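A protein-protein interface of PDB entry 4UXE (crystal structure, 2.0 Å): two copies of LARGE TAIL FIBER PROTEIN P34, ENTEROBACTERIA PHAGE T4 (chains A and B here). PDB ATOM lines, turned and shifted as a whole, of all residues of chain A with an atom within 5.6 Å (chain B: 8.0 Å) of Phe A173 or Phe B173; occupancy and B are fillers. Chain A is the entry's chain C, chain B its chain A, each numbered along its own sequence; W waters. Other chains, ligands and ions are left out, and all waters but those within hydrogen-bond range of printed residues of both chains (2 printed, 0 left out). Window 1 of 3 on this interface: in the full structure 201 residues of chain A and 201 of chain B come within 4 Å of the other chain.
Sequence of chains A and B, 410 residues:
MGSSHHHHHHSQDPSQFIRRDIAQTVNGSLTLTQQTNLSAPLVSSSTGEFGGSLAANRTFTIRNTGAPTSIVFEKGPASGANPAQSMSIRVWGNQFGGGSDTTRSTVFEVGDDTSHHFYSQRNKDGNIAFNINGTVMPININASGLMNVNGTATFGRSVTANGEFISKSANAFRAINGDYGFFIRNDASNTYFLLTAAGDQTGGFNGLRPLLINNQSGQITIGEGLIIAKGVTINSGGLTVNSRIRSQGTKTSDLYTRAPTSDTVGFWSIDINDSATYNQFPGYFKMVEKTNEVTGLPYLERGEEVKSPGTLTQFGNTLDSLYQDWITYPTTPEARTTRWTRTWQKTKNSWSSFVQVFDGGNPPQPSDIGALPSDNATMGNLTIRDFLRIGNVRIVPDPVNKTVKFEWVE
The backbone NH (N) of Phe A165 sits at hydrogen-bond distance from the backbone carbonyl oxygen (O) of Ala B172 (2.9 Å).
NE of Arg B174 lies within salt-bridge range of OE2 of Glu A164.
O of Phe A165 lies within hydrogen-bond range of N of Arg B174 (2.8 Å).
N of Ser A167 lies within hydrogen-bond range of O of Arg B174 (2.9 Å).
The backbone NH (N) of Ile B176 lies within hydrogen-bond range of the backbone carbonyl oxygen (O) of Ser A167 (2.9 Å).
OG of Ser B167 sits at hydrogen-bond distance from N of Ser B169, 3.1 Å away.
The backbone NH (N) of Ala B175 sits at hydrogen-bond distance from the backbone carbonyl oxygen (O) of Phe B182 (2.7 Å).
The backbone NH (N) of Ala A172 sits at hydrogen-bond distance from the backbone carbonyl oxygen (O) of Ile A184, at 2.9 Å.
Asn B171 touches Glu A164 (O to CB, 3.3 Å).
Glu A164 touches Ala B172.
Phe A165 touches Ile B166.
CD2 of Phe A165 touches CE1 of Phe B173, 3.4 Å away.
CG2 of Ile A166 touches CD1 of Ile B176, at 3.6 Å.
Ala B175 touches Ser A167.
CB of Ala A172 touches CB of Ala B175 (3.4 Å).
CD1 of Phe B173 touches CE1 of Phe A173 (3.7 Å).
CE2 of Phe A173 touches N of Ala B175, 3.99 Å away.
Of chain A, only Phe A165 (3.4 Å) and Phe A173 (3.7 Å) come within 4 Å of Phe B173.
Of chain B, only Ala B175 (3.4 Å) comes within 4 Å of Ala A172.
Printed residues of chain A within 4 Å of Arg B174: Glu A164, Phe A165, Ile A166, Ser A167 and Phe A173.
Of the printed residues of chain A, Asn B171 touches Glu A164.
Printed residues of chain A within 4 Å of Ser B167: Phe A165.
Printed residues of chain A within 4 Å of Ala B175: Ser A167, Ala A172 and Phe A173.
The nearest printed residue of chain B that does not touch Phe A173 is Ala B172 (5.8 Å).
The nearest residue of chain A that does not touch Phe B173 is Glu A164 (4.4 Å).
Of the 23 printed residues of chain B, 10 touch a printed residue of chain A.
Printed residues of chain B that touch a printed residue of chain A: Phe B165, Ile B166, Ser B167, Ser B169, Asn B171, Ala B172, Phe B173, Arg B174, Ala B175 and Ile B176.
Hydrophobic or aromatic side chains of chain B that line the printed part of chain A: Phe B165, Phe B173, Ala B175 and Ile B176.
Along chain B the printed residues that touch a printed residue of chain A span positions 165 to 176.
Of the 12 printed residues of chain A, 6 touch a printed residue of chain B.
Hydrophobic or aromatic side chains of chain A that line the printed part of chain B: Phe A165, Ile A166, Ala A172 and Phe A173.
Glu A164 touches Arg B174, but with the chains exchanged Arg A174 does not touch Glu B164 (9.0 Å).
Phe A165 touches Ser B167, but with the chains exchanged Ser A167 does not touch Phe B165 (9.7 Å).
Phe A173 touches Arg B174, but with the chains exchanged Arg A174 does not touch Phe B173 (8.6 Å).
Water W2 bridges the side-chain carboxylate (OE1) of Glu A164 and the guanidinium group (NE) of Arg B174.
Water W1 lies within hydrogen-bond range of OE1 of Glu A164, ND2 of Asn B171 and NH2 of Arg B174.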
ATOM      1  N   GLU A 164      22.331 -13.977 -35.163  1.00  0.00           N
ATOM      2  CA  GLU A 164      22.660 -14.510 -33.843  1.00  0.00           C
ATOM      3  C   GLU A 164      21.460 -14.475 -32.905  1.00  0.00           C
ATOM      4  O   GLU A 164      20.620 -13.565 -33.005  1.00  0.00           O
ATOM      5  CB  GLU A 164      23.760 -13.598 -33.272  1.00  0.00           C
ATOM      6  CG  GLU A 164      24.372 -14.005 -31.938  1.00  0.00           C
ATOM      7  CD  GLU A 164      25.620 -13.164 -31.613  1.00  0.00           C
ATOM      8  OE1 GLU A 164      25.651 -11.958 -31.963  1.00  0.00           O
ATOM      9  OE2 GLU A 164      26.558 -13.709 -30.989  1.00  0.00           O
ATOM     10  N   PHE A 165      21.379 -15.451 -31.995  1.00  0.00           N
ATOM     11  CA  PHE A 165      20.419 -15.400 -30.880  1.00  0.00           C
ATOM     12  C   PHE A 165      21.140 -14.803 -29.686  1.00  0.00           C
ATOM     13  O   PHE A 165      22.199 -15.285 -29.307  1.00  0.00           O
ATOM     14  CB  PHE A 165      19.896 -16.804 -30.496  1.00  0.00           C
ATOM     15  CG  PHE A 165      18.953 -17.430 -31.522  1.00  0.00           C
ATOM     16  CD1 PHE A 165      17.591 -17.158 -31.493  1.00  0.00           C
ATOM     17  CD2 PHE A 165      19.436 -18.303 -32.484  1.00  0.00           C
ATOM     18  CE1 PHE A 165      16.723 -17.731 -32.428  1.00  0.00           C
ATOM     19  CE2 PHE A 165      18.575 -18.909 -33.418  1.00  0.00           C
ATOM     20  CZ  PHE A 165      17.221 -18.605 -33.394  1.00  0.00           C
ATOM     21  N   ILE A 166      20.577 -13.767 -29.077  1.00  0.00           N
ATOM     22  CA  ILE A 166      21.205 -13.108 -27.945  1.00  0.00           C
ATOM     23  C   ILE A 166      20.212 -13.049 -26.799  1.00  0.00           C
ATOM     24  O   ILE A 166      19.073 -12.607 -26.996  1.00  0.00           O
ATOM     25  CB  ILE A 166      21.604 -11.675 -28.299  1.00  0.00           C
ATOM     26  CG1 ILE A 166      22.616 -11.665 -29.464  1.00  0.00           C
ATOM     27  CG2 ILE A 166      22.174 -10.967 -27.065  1.00  0.00           C
ATOM     28  CD1 ILE A 166      22.157 -10.901 -30.675  1.00  0.00           C
ATOM     29  N   SER A 167      20.625 -13.505 -25.619  1.00  0.00           N
ATOM     30  CA  SER A 167      19.802 -13.385 -24.417  1.00  0.00           C
ATOM     31  C   SER A 167      20.504 -12.472 -23.419  1.00  0.00           C
ATOM     32  O   SER A 167      21.727 -12.542 -23.250  1.00  0.00           O
ATOM     33  CB  SER A 167      19.524 -14.743 -23.783  1.00  0.00           C
ATOM     34  OG  SER A 167      18.812 -14.564 -22.571  1.00  0.00           O
ATOM     35  N   ASN A 171      20.060 -16.743 -16.824  1.00  0.00           N
ATOM     36  CA  ASN A 171      19.722 -18.034 -17.449  1.00  0.00           C
ATOM     37  C   ASN A 171      19.338 -17.761 -18.894  1.00  0.00           C
ATOM     38  O   ASN A 171      18.283 -17.157 -19.165  1.00  0.00           O
ATOM     39  CB  ASN A 171      18.592 -18.714 -16.686  1.00  0.00           C
ATOM     40  CG  ASN A 171      19.009 -19.120 -15.277  1.00  0.00           C
ATOM     41  OD1 ASN A 171      20.200 -19.097 -14.951  1.00  0.00           O
ATOM     42  ND2 ASN A 171      18.040 -19.479 -14.437  1.00  0.00           N
ATOM     43  N   ALA A 172      20.207 -18.176 -19.817  1.00  0.00           N
ATOM     44  CA  ALA A 172      20.159 -17.720 -21.205  1.00  0.00           C
ATOM     45  C   ALA A 172      19.566 -18.701 -22.212  1.00  0.00           C
ATOM     46  O   ALA A 172      18.720 -18.312 -23.030  1.00  0.00           O
ATOM     47  CB  ALA A 172      21.555 -17.272 -21.664  1.00  0.00           C
ATOM     48  N   PHE A 173      20.019 -19.954 -22.171  1.00  0.00           N
ATOM     49  CA  PHE A 173      19.593 -20.979 -23.123  1.00  0.00           C
ATOM     50  C   PHE A 173      19.333 -22.261 -22.332  1.00  0.00           C
ATOM     51  O   PHE A 173      20.194 -22.708 -21.562  1.00  0.00           O
ATOM     52  CB  PHE A 173      20.668 -21.217 -24.200  1.00  0.00           C
ATOM     53  CG  PHE A 173      21.003 -19.973 -25.002  1.00  0.00           C
ATOM     54  CD1 PHE A 173      20.207 -19.593 -26.078  1.00  0.00           C
ATOM     55  CD2 PHE A 173      22.083 -19.161 -24.647  1.00  0.00           C
ATOM     56  CE1 PHE A 173      20.484 -18.414 -26.804  1.00  0.00           C
ATOM     57  CE2 PHE A 173      22.370 -17.983 -25.367  1.00  0.00           C
ATOM     58  CZ  PHE A 173      21.561 -17.617 -26.444  1.00  0.00           C
ATOM     59  N   ARG A 174      18.147 -22.831 -22.509  1.00  0.00           N
ATOM     60  CA  ARG A 174      17.718 -23.981 -21.747  1.00  0.00           C
ATOM     61  C   ARG A 174      17.142 -25.027 -22.681  1.00  0.00           C
ATOM     62  O   ARG A 174      16.306 -24.708 -23.552  1.00  0.00           O
ATOM     63  CB  ARG A 174      16.656 -23.580 -20.712  1.00  0.00           C
ATOM     64  CG  ARG A 174      16.103 -24.768 -19.890  1.00  0.00           C
ATOM     65  CD  ARG A 174      15.121 -24.317 -18.800  1.00  0.00           C
ATOM     66  NE  ARG A 174      15.691 -23.288 -17.905  1.00  0.00           N
ATOM     67  CZ  ARG A 174      15.825 -23.402 -16.586  1.00  0.00           C
ATOM     68  NH1 ARG A 174      15.452 -24.521 -15.956  1.00  0.00           N
ATOM     69  NH2 ARG A 174      16.334 -22.386 -15.884  1.00  0.00           N
ATOM     70  N   ALA A 175      17.599 -26.268 -22.508  1.00  0.00           N
ATOM     71  CA  ALA A 175      17.090 -27.408 -23.276  1.00  0.00           C
ATOM     72  C   ALA A 175      16.397 -28.353 -22.294  1.00  0.00           C
ATOM     73  O   ALA A 175      17.042 -28.899 -21.388  1.00  0.00           O
ATOM     74  CB  ALA A 175      18.254 -28.119 -23.986  1.00  0.00           C
ATOM     75  N   PHE A 182      18.546 -28.572 -18.841  1.00  0.00           N
ATOM     76  CA  PHE A 182      19.945 -28.211 -18.928  1.00  0.00           C
ATOM     77  C   PHE A 182      20.007 -26.767 -19.398  1.00  0.00           C
ATOM     78  O   PHE A 182      19.321 -26.410 -20.356  1.00  0.00           O
ATOM     79  CB  PHE A 182      20.629 -29.075 -19.978  1.00  0.00           C
ATOM     80  CG  PHE A 182      22.011 -28.604 -20.318  1.00  0.00           C
ATOM     81  CD1 PHE A 182      23.102 -28.988 -19.531  1.00  0.00           C
ATOM     82  CD2 PHE A 182      22.223 -27.751 -21.400  1.00  0.00           C
ATOM     83  CE1 PHE A 182      24.384 -28.530 -19.836  1.00  0.00           C
ATOM     84  CE2 PHE A 182      23.498 -27.294 -21.713  1.00  0.00           C
ATOM     85  CZ  PHE A 182      24.576 -27.679 -20.933  1.00  0.00           C
ATOM     86  N   PHE A 183      20.824 -25.940 -18.762  1.00  0.00           N
ATOM     87  CA  PHE A 183      20.901 -24.537 -19.159  1.00  0.00           C
ATOM     88  C   PHE A 183      22.250 -23.883 -19.012  1.00  0.00           C
ATOM     89  O   PHE A 183      23.078 -24.314 -18.200  1.00  0.00           O
ATOM     90  CB  PHE A 183      19.784 -23.677 -18.520  1.00  0.00           C
ATOM     91  CG  PHE A 183      19.774 -23.648 -17.023  1.00  0.00           C
ATOM     92  CD1 PHE A 183      19.264 -24.719 -16.294  1.00  0.00           C
ATOM     93  CD2 PHE A 183      20.203 -22.500 -16.337  1.00  0.00           C
ATOM     94  CE1 PHE A 183      19.205 -24.685 -14.895  1.00  0.00           C
ATOM     95  CE2 PHE A 183      20.149 -22.439 -14.932  1.00  0.00           C
ATOM     96  CZ  PHE A 183      19.657 -23.533 -14.207  1.00  0.00           C
ATOM     97  N   ILE A 184      22.467 -22.865 -19.840  1.00  0.00           N
ATOM     98  CA  ILE A 184      23.668 -22.063 -19.792  1.00  0.00           C
ATOM     99  C   ILE A 184      23.307 -20.766 -19.065  1.00  0.00           C
ATOM    100  O   ILE A 184      22.340 -20.077 -19.430  1.00  0.00           O
ATOM    101  CB  ILE A 184      24.182 -21.742 -21.202  1.00  0.00           C
ATOM    102  CG1 ILE A 184      24.552 -23.045 -21.952  1.00  0.00           C
ATOM    103  CG2 ILE A 184      25.339 -20.719 -21.125  1.00  0.00           C
ATOM    104  CD1 ILE A 184      24.750 -22.874 -23.476  1.00  0.00           C
ATOM    105  N   VAL B 159      11.446 -16.799 -24.541  1.00  0.00           N
ATOM    106  CA  VAL B 159      11.087 -17.329 -25.837  1.00  0.00           C
ATOM    107  C   VAL B 159      11.202 -18.837 -25.753  1.00  0.00           C
ATOM    108  O   VAL B 159      12.295 -19.364 -25.586  1.00  0.00           O
ATOM    109  CB  VAL B 159      12.023 -16.794 -26.933  1.00  0.00           C
ATOM    110  CG1 VAL B 159      11.672 -17.412 -28.303  1.00  0.00           C
ATOM    111  CG2 VAL B 159      11.963 -15.260 -26.984  1.00  0.00           C
ATOM    112  N   GLU B 164      13.558 -26.945 -32.397  1.00  0.00           N
ATOM    113  CA  GLU B 164      14.945 -26.551 -32.270  1.00  0.00           C
ATOM    114  C   GLU B 164      15.138 -25.068 -32.628  1.00  0.00           C
ATOM    115  O   GLU B 164      14.428 -24.544 -33.502  1.00  0.00           O
ATOM    116  CB  GLU B 164      15.718 -27.422 -33.266  1.00  0.00           C
ATOM    117  CG  GLU B 164      17.227 -27.359 -33.200  1.00  0.00           C
ATOM    118  CD  GLU B 164      17.875 -28.432 -34.079  1.00  0.00           C
ATOM    119  OE1 GLU B 164      17.241 -28.885 -35.075  1.00  0.00           O
ATOM    120  OE2 GLU B 164      19.024 -28.827 -33.761  1.00  0.00           O
ATOM    121  N   PHE B 165      16.083 -24.396 -31.958  1.00  0.00           N
ATOM    122  CA  PHE B 165      16.565 -23.073 -32.393  1.00  0.00           C
ATOM    123  C   PHE B 165      17.795 -23.286 -33.275  1.00  0.00           C
ATOM    124  O   PHE B 165      18.760 -23.959 -32.871  1.00  0.00           O
ATOM    125  CB  PHE B 165      16.976 -22.190 -31.216  1.00  0.00           C
ATOM    126  CG  PHE B 165      15.829 -21.761 -30.339  1.00  0.00           C
ATOM    127  CD1 PHE B 165      15.436 -22.543 -29.260  1.00  0.00           C
ATOM    128  CD2 PHE B 165      15.162 -20.568 -30.590  1.00  0.00           C
ATOM    129  CE1 PHE B 165      14.379 -22.149 -28.435  1.00  0.00           C
ATOM    130  CE2 PHE B 165      14.094 -20.164 -29.783  1.00  0.00           C
ATOM    131  CZ  PHE B 165      13.709 -20.948 -28.703  1.00  0.00           C
ATOM    132  N   ILE B 166      17.785 -22.700 -34.464  1.00  0.00           N
ATOM    133  CA  ILE B 166      18.882 -22.915 -35.426  1.00  0.00           C
ATOM    134  C   ILE B 166      19.385 -21.551 -35.862  1.00  0.00           C
ATOM    135  O   ILE B 166      18.587 -20.723 -36.296  1.00  0.00           O
ATOM    136  CB  ILE B 166      18.387 -23.731 -36.634  1.00  0.00           C
ATOM    137  CG1 ILE B 166      17.771 -25.051 -36.156  1.00  0.00           C
ATOM    138  CG2 ILE B 166      19.526 -23.955 -37.667  1.00  0.00           C
ATOM    139  CD1 ILE B 166      16.477 -25.383 -36.777  1.00  0.00           C
ATOM    140  N   SER B 167      20.685 -21.298 -35.709  1.00  0.00           N
ATOM    141  CA  SER B 167      21.296 -20.089 -36.248  1.00  0.00           C
ATOM    142  C   SER B 167      22.192 -20.435 -37.443  1.00  0.00           C
ATOM    143  O   SER B 167      22.900 -21.456 -37.418  1.00  0.00           O
ATOM    144  CB  SER B 167      22.118 -19.354 -35.181  1.00  0.00           C
ATOM    145  OG  SER B 167      22.769 -18.213 -35.762  1.00  0.00           O
ATOM    146  N   LYS B 168      22.163 -19.592 -38.481  1.00  0.00           N
ATOM    147  CA  LYS B 168      23.071 -19.708 -39.625  1.00  0.00           C
ATOM    148  C   LYS B 168      24.217 -18.695 -39.534  1.00  0.00           C
ATOM    149  O   LYS B 168      24.999 -18.529 -40.480  1.00  0.00           O
ATOM    150  CB  LYS B 168      22.309 -19.505 -40.941  1.00  0.00           C
ATOM    151  CG  LYS B 168      21.086 -20.385 -41.147  1.00  0.00           C
ATOM    152  CD  LYS B 168      21.451 -21.824 -41.338  1.00  0.00           C
ATOM    153  CE  LYS B 168      20.219 -22.646 -41.705  1.00  0.00           C
ATOM    154  NZ  LYS B 168      19.635 -22.247 -43.016  1.00  0.00           N
ATOM    155  N   SER B 169      24.299 -18.009 -38.404  1.00  0.00           N
ATOM    156  CA  SER B 169      25.327 -17.012 -38.139  1.00  0.00           C
ATOM    157  C   SER B 169      26.549 -17.679 -37.474  1.00  0.00           C
ATOM    158  O   SER B 169      26.370 -18.527 -36.599  1.00  0.00           O
ATOM    159  CB  SER B 169      24.740 -15.958 -37.198  1.00  0.00           C
ATOM    160  OG  SER B 169      25.700 -15.017 -36.752  1.00  0.00           O
ATOM    161  N   ALA B 170      27.771 -17.310 -37.879  1.00  0.00           N
ATOM    162  CA  ALA B 170      28.982 -17.880 -37.251  1.00  0.00           C
ATOM    163  C   ALA B 170      28.896 -17.715 -35.732  1.00  0.00           C
ATOM    164  O   ALA B 170      28.951 -18.694 -35.012  1.00  0.00           O
ATOM    165  CB  ALA B 170      30.256 -17.222 -37.799  1.00  0.00           C
ATOM    166  N   ASN B 171      28.708 -16.481 -35.253  1.00  0.00           N
ATOM    167  CA  ASN B 171      28.334 -16.265 -33.855  1.00  0.00           C
ATOM    168  C   ASN B 171      26.862 -16.593 -33.728  1.00  0.00           C
ATOM    169  O   ASN B 171      26.008 -15.851 -34.243  1.00  0.00           O
ATOM    170  CB  ASN B 171      28.619 -14.822 -33.431  1.00  0.00           C
ATOM    171  CG  ASN B 171      30.097 -14.487 -33.496  1.00  0.00           C
ATOM    172  OD1 ASN B 171      30.935 -15.387 -33.548  1.00  0.00           O
ATOM    173  ND2 ASN B 171      30.429 -13.199 -33.503  1.00  0.00           N
ATOM    174  N   ALA B 172      26.557 -17.706 -33.065  1.00  0.00           N
ATOM    175  CA  ALA B 172      25.213 -18.288 -33.110  1.00  0.00           C
ATOM    176  C   ALA B 172      24.370 -18.035 -31.852  1.00  0.00           C
ATOM    177  O   ALA B 172      23.184 -17.711 -31.964  1.00  0.00           O
ATOM    178  CB  ALA B 172      25.299 -19.789 -33.410  1.00  0.00           C
ATOM    179  N   PHE B 173      24.964 -18.205 -30.664  1.00  0.00           N
ATOM    180  CA  PHE B 173      24.202 -18.086 -29.411  1.00  0.00           C
ATOM    181  C   PHE B 173      25.015 -17.286 -28.418  1.00  0.00           C
ATOM    182  O   PHE B 173      26.154 -17.643 -28.137  1.00  0.00           O
ATOM    183  CB  PHE B 173      23.862 -19.469 -28.838  1.00  0.00           C
ATOM    184  CG  PHE B 173      23.041 -20.306 -29.760  1.00  0.00           C
ATOM    185  CD1 PHE B 173      21.661 -20.108 -29.867  1.00  0.00           C
ATOM    186  CD2 PHE B 173      23.645 -21.255 -30.586  1.00  0.00           C
ATOM    187  CE1 PHE B 173      20.878 -20.877 -30.782  1.00  0.00           C
ATOM    188  CE2 PHE B 173      22.886 -22.009 -31.487  1.00  0.00           C
ATOM    189  CZ  PHE B 173      21.500 -21.807 -31.589  1.00  0.00           C
ATOM    190  N   ARG B 174      24.445 -16.217 -27.875  1.00  0.00           N
ATOM    191  CA  ARG B 174      25.190 -15.332 -26.986  1.00  0.00           C
ATOM    192  C   ARG B 174      24.392 -15.062 -25.718  1.00  0.00           C
ATOM    193  O   ARG B 174      23.183 -14.772 -25.783  1.00  0.00           O
ATOM    194  CB  ARG B 174      25.543 -14.015 -27.702  1.00  0.00           C
ATOM    195  CG  ARG B 174      26.224 -12.968 -26.799  1.00  0.00           C
ATOM    196  CD  ARG B 174      26.576 -11.716 -27.596  1.00  0.00           C
ATOM    197  NE  ARG B 174      27.332 -12.015 -28.823  1.00  0.00           N
ATOM    198  CZ  ARG B 174      28.544 -11.533 -29.115  1.00  0.00           C
ATOM    199  NH1 ARG B 174      29.181 -10.705 -28.275  1.00  0.00           N
ATOM    200  NH2 ARG B 174      29.131 -11.887 -30.255  1.00  0.00           N
ATOM    201  N   ALA B 175      25.081 -15.164 -24.574  1.00  0.00           N
ATOM    202  CA  ALA B 175      24.528 -14.837 -23.265  1.00  0.00           C
ATOM    203  C   ALA B 175      25.264 -13.615 -22.700  1.00  0.00           C
ATOM    204  O   ALA B 175      26.464 -13.686 -22.422  1.00  0.00           O
ATOM    205  CB  ALA B 175      24.691 -16.017 -22.320  1.00  0.00           C
ATOM    206  N   ILE B 176      24.539 -12.512 -22.526  1.00  0.00           N
ATOM    207  CA  ILE B 176      25.106 -11.271 -22.023  1.00  0.00           C
ATOM    208  C   ILE B 176      24.664 -11.048 -20.589  1.00  0.00           C
ATOM    209  O   ILE B 176      23.468 -11.092 -20.284  1.00  0.00           O
ATOM    210  CB  ILE B 176      24.679 -10.065 -22.892  1.00  0.00           C
ATOM    211  CG1 ILE B 176      25.352 -10.135 -24.276  1.00  0.00           C
ATOM    212  CG2 ILE B 176      24.980  -8.719 -22.164  1.00  0.00           C
ATOM    213  CD1 ILE B 176      24.739  -9.143 -25.287  1.00  0.00           C
ATOM    214  N   GLY B 181      29.860 -10.694 -22.641  1.00  0.00           N
ATOM    215  CA  GLY B 181      29.116 -11.571 -23.513  1.00  0.00           C
ATOM    216  C   GLY B 181      29.853 -12.897 -23.588  1.00  0.00           C
ATOM    217  O   GLY B 181      31.073 -12.939 -23.753  1.00  0.00           O
ATOM    218  N   PHE B 182      29.116 -13.981 -23.437  1.00  0.00           N
ATOM    219  CA  PHE B 182      29.650 -15.313 -23.699  1.00  0.00           C
ATOM    220  C   PHE B 182      28.952 -15.820 -24.946  1.00  0.00           C
ATOM    221  O   PHE B 182      27.727 -15.663 -25.069  1.00  0.00           O
ATOM    222  CB  PHE B 182      29.326 -16.253 -22.522  1.00  0.00           C
ATOM    223  CG  PHE B 182      29.565 -17.687 -22.836  1.00  0.00           C
ATOM    224  CD1 PHE B 182      30.849 -18.219 -22.740  1.00  0.00           C
ATOM    225  CD2 PHE B 182      28.521 -18.497 -23.292  1.00  0.00           C
ATOM    226  CE1 PHE B 182      31.090 -19.554 -23.076  1.00  0.00           C
ATOM    227  CE2 PHE B 182      28.758 -19.835 -23.621  1.00  0.00           C
ATOM    228  CZ  PHE B 182      30.049 -20.357 -23.504  1.00  0.00           C
ATOM    229  N   PHE B 183      29.685 -16.433 -25.875  1.00  0.00           N
ATOM    230  CA  PHE B 183      29.008 -16.928 -27.059  1.00  0.00           C
ATOM    231  C   PHE B 183      29.601 -18.170 -27.706  1.00  0.00           C
ATOM    232  O   PHE B 183      30.791 -18.494 -27.542  1.00  0.00           O
ATOM    233  CB  PHE B 183      28.779 -15.817 -28.104  1.00  0.00           C
ATOM    234  CG  PHE B 183      30.044 -15.177 -28.638  1.00  0.00           C
ATOM    235  CD1 PHE B 183      30.739 -14.225 -27.879  1.00  0.00           C
ATOM    236  CD2 PHE B 183      30.498 -15.496 -29.924  1.00  0.00           C
ATOM    237  CE1 PHE B 183      31.881 -13.591 -28.399  1.00  0.00           C
ATOM    238  CE2 PHE B 183      31.648 -14.890 -30.447  1.00  0.00           C
ATOM    239  CZ  PHE B 183      32.336 -13.931 -29.690  1.00  0.00           C
ATOM    240  N   ILE B 184      28.729 -18.872 -28.418  1.00  0.00           N
ATOM    241  CA  ILE B 184      29.102 -20.037 -29.200  1.00  0.00           C
ATOM    242  C   ILE B 184      29.245 -19.615 -30.649  1.00  0.00           C
ATOM    243  O   ILE B 184      28.306 -19.040 -31.239  1.00  0.00           O
ATOM    244  CB  ILE B 184      28.053 -21.174 -29.050  1.00  0.00           C
ATOM    245  CG1 ILE B 184      27.900 -21.549 -27.560  1.00  0.00           C
ATOM    246  CG2 ILE B 184      28.424 -22.383 -29.912  1.00  0.00           C
ATOM    247  CD1 ILE B 184      26.752 -22.539 -27.274  1.00  0.00           C
ATOM    248  N   ARG B 185      30.423 -19.900 -31.215  1.00  0.00           N
ATOM    249  CA  ARG B 185      30.765 -19.536 -32.585  1.00  0.00           C
ATOM    250  C   ARG B 185      31.172 -20.786 -33.379  1.00  0.00           C
ATOM    251  O   ARG B 185      32.158 -21.436 -33.035  1.00  0.00           O
ATOM    252  CB  ARG B 185      31.928 -18.515 -32.559  1.00  0.00           C
ATOM    253  CG  ARG B 185      32.474 -18.182 -33.951  1.00  0.00           C
ATOM    254  CD  ARG B 185      33.638 -17.173 -33.865  1.00  0.00           C
ATOM    255  NE  ARG B 185      34.214 -16.923 -35.190  1.00  0.00           N
ATOM    256  CZ  ARG B 185      33.718 -16.063 -36.083  1.00  0.00           C
ATOM    257  NH1 ARG B 185      32.608 -15.365 -35.817  1.00  0.00           N
ATOM    258  NH2 ARG B 185      34.335 -15.901 -37.252  1.00  0.00           N
ATOM    259  N   ASN B 186      30.413 -21.138 -34.416  1.00  0.00           N
ATOM    260  CA  ASN B 186      30.822 -22.194 -35.334  1.00  0.00           C
ATOM    261  C   ASN B 186      31.444 -21.481 -36.512  1.00  0.00           C
ATOM    262  O   ASN B 186      30.730 -20.819 -37.282  1.00  0.00           O
ATOM    263  CB  ASN B 186      29.620 -23.040 -35.780  1.00  0.00           C
ATOM    264  CG  ASN B 186      29.991 -24.091 -36.805  1.00  0.00           C
ATOM    265  OD1 ASN B 186      31.136 -24.153 -37.273  1.00  0.00           O
ATOM    266  ND2 ASN B 186      29.023 -24.925 -37.173  1.00  0.00           N
ATOM    267  N   TYR B 192      33.599 -22.755 -31.152  1.00  0.00           N
ATOM    268  CA  TYR B 192      34.290 -22.139 -30.018  1.00  0.00           C
ATOM    269  C   TYR B 192      33.279 -21.664 -28.996  1.00  0.00           C
ATOM    270  O   TYR B 192      32.184 -21.213 -29.370  1.00  0.00           O
ATOM    271  CB  TYR B 192      35.070 -20.879 -30.477  1.00  0.00           C
ATOM    272  CG  TYR B 192      36.196 -21.095 -31.464  1.00  0.00           C
ATOM    273  CD1 TYR B 192      35.934 -21.309 -32.818  1.00  0.00           C
ATOM    274  CD2 TYR B 192      37.543 -21.062 -31.042  1.00  0.00           C
ATOM    275  CE1 TYR B 192      36.977 -21.490 -33.746  1.00  0.00           C
ATOM    276  CE2 TYR B 192      38.605 -21.259 -31.967  1.00  0.00           C
ATOM    277  CZ  TYR B 192      38.300 -21.476 -33.309  1.00  0.00           C
ATOM    278  OH  TYR B 192      39.297 -21.659 -34.236  1.00  0.00           O
ATOM    279  N   PHE B 193      33.656 -21.727 -27.717  1.00  0.00           N
ATOM    280  CA  PHE B 193      32.956 -21.023 -26.649  1.00  0.00           C
ATOM    281  C   PHE B 193      33.843 -19.808 -26.338  1.00  0.00           C
ATOM    282  O   PHE B 193      35.018 -19.981 -25.947  1.00  0.00           O
ATOM    283  CB  PHE B 193      32.838 -21.893 -25.394  1.00  0.00           C
ATOM    284  CG  PHE B 193      31.987 -23.130 -25.566  1.00  0.00           C
ATOM    285  CD1 PHE B 193      31.220 -23.334 -26.692  1.00  0.00           C
ATOM    286  CD2 PHE B 193      31.936 -24.080 -24.551  1.00  0.00           C
ATOM    287  CE1 PHE B 193      30.411 -24.479 -26.840  1.00  0.00           C
ATOM    288  CE2 PHE B 193      31.138 -25.227 -24.683  1.00  0.00           C
ATOM    289  CZ  PHE B 193      30.368 -25.412 -25.844  1.00  0.00           C
ATOM    290  N   LEU B 194      33.331 -18.600 -26.567  1.00  0.00           N
ATOM    291  CA  LEU B 194      34.194 -17.411 -26.542  1.00  0.00           C
ATOM    292  C   LEU B 194      33.647 -16.336 -25.622  1.00  0.00           C
ATOM    293  O   LEU B 194      32.496 -16.413 -25.181  1.00  0.00           O
ATOM    294  CB  LEU B 194      34.361 -16.844 -27.960  1.00  0.00           C
ATOM    295  CG  LEU B 194      35.049 -17.776 -28.968  1.00  0.00           C
ATOM    296  CD1 LEU B 194      34.860 -17.262 -30.367  1.00  0.00           C
ATOM    297  CD2 LEU B 194      36.542 -17.908 -28.647  1.00  0.00           C
HETATM  298  O   HOH W   1      28.022 -11.418 -33.409  1.00  0.00           O
HETATM  299  O   HOH W   2      26.002  -9.624 -30.502  1.00  0.00           O
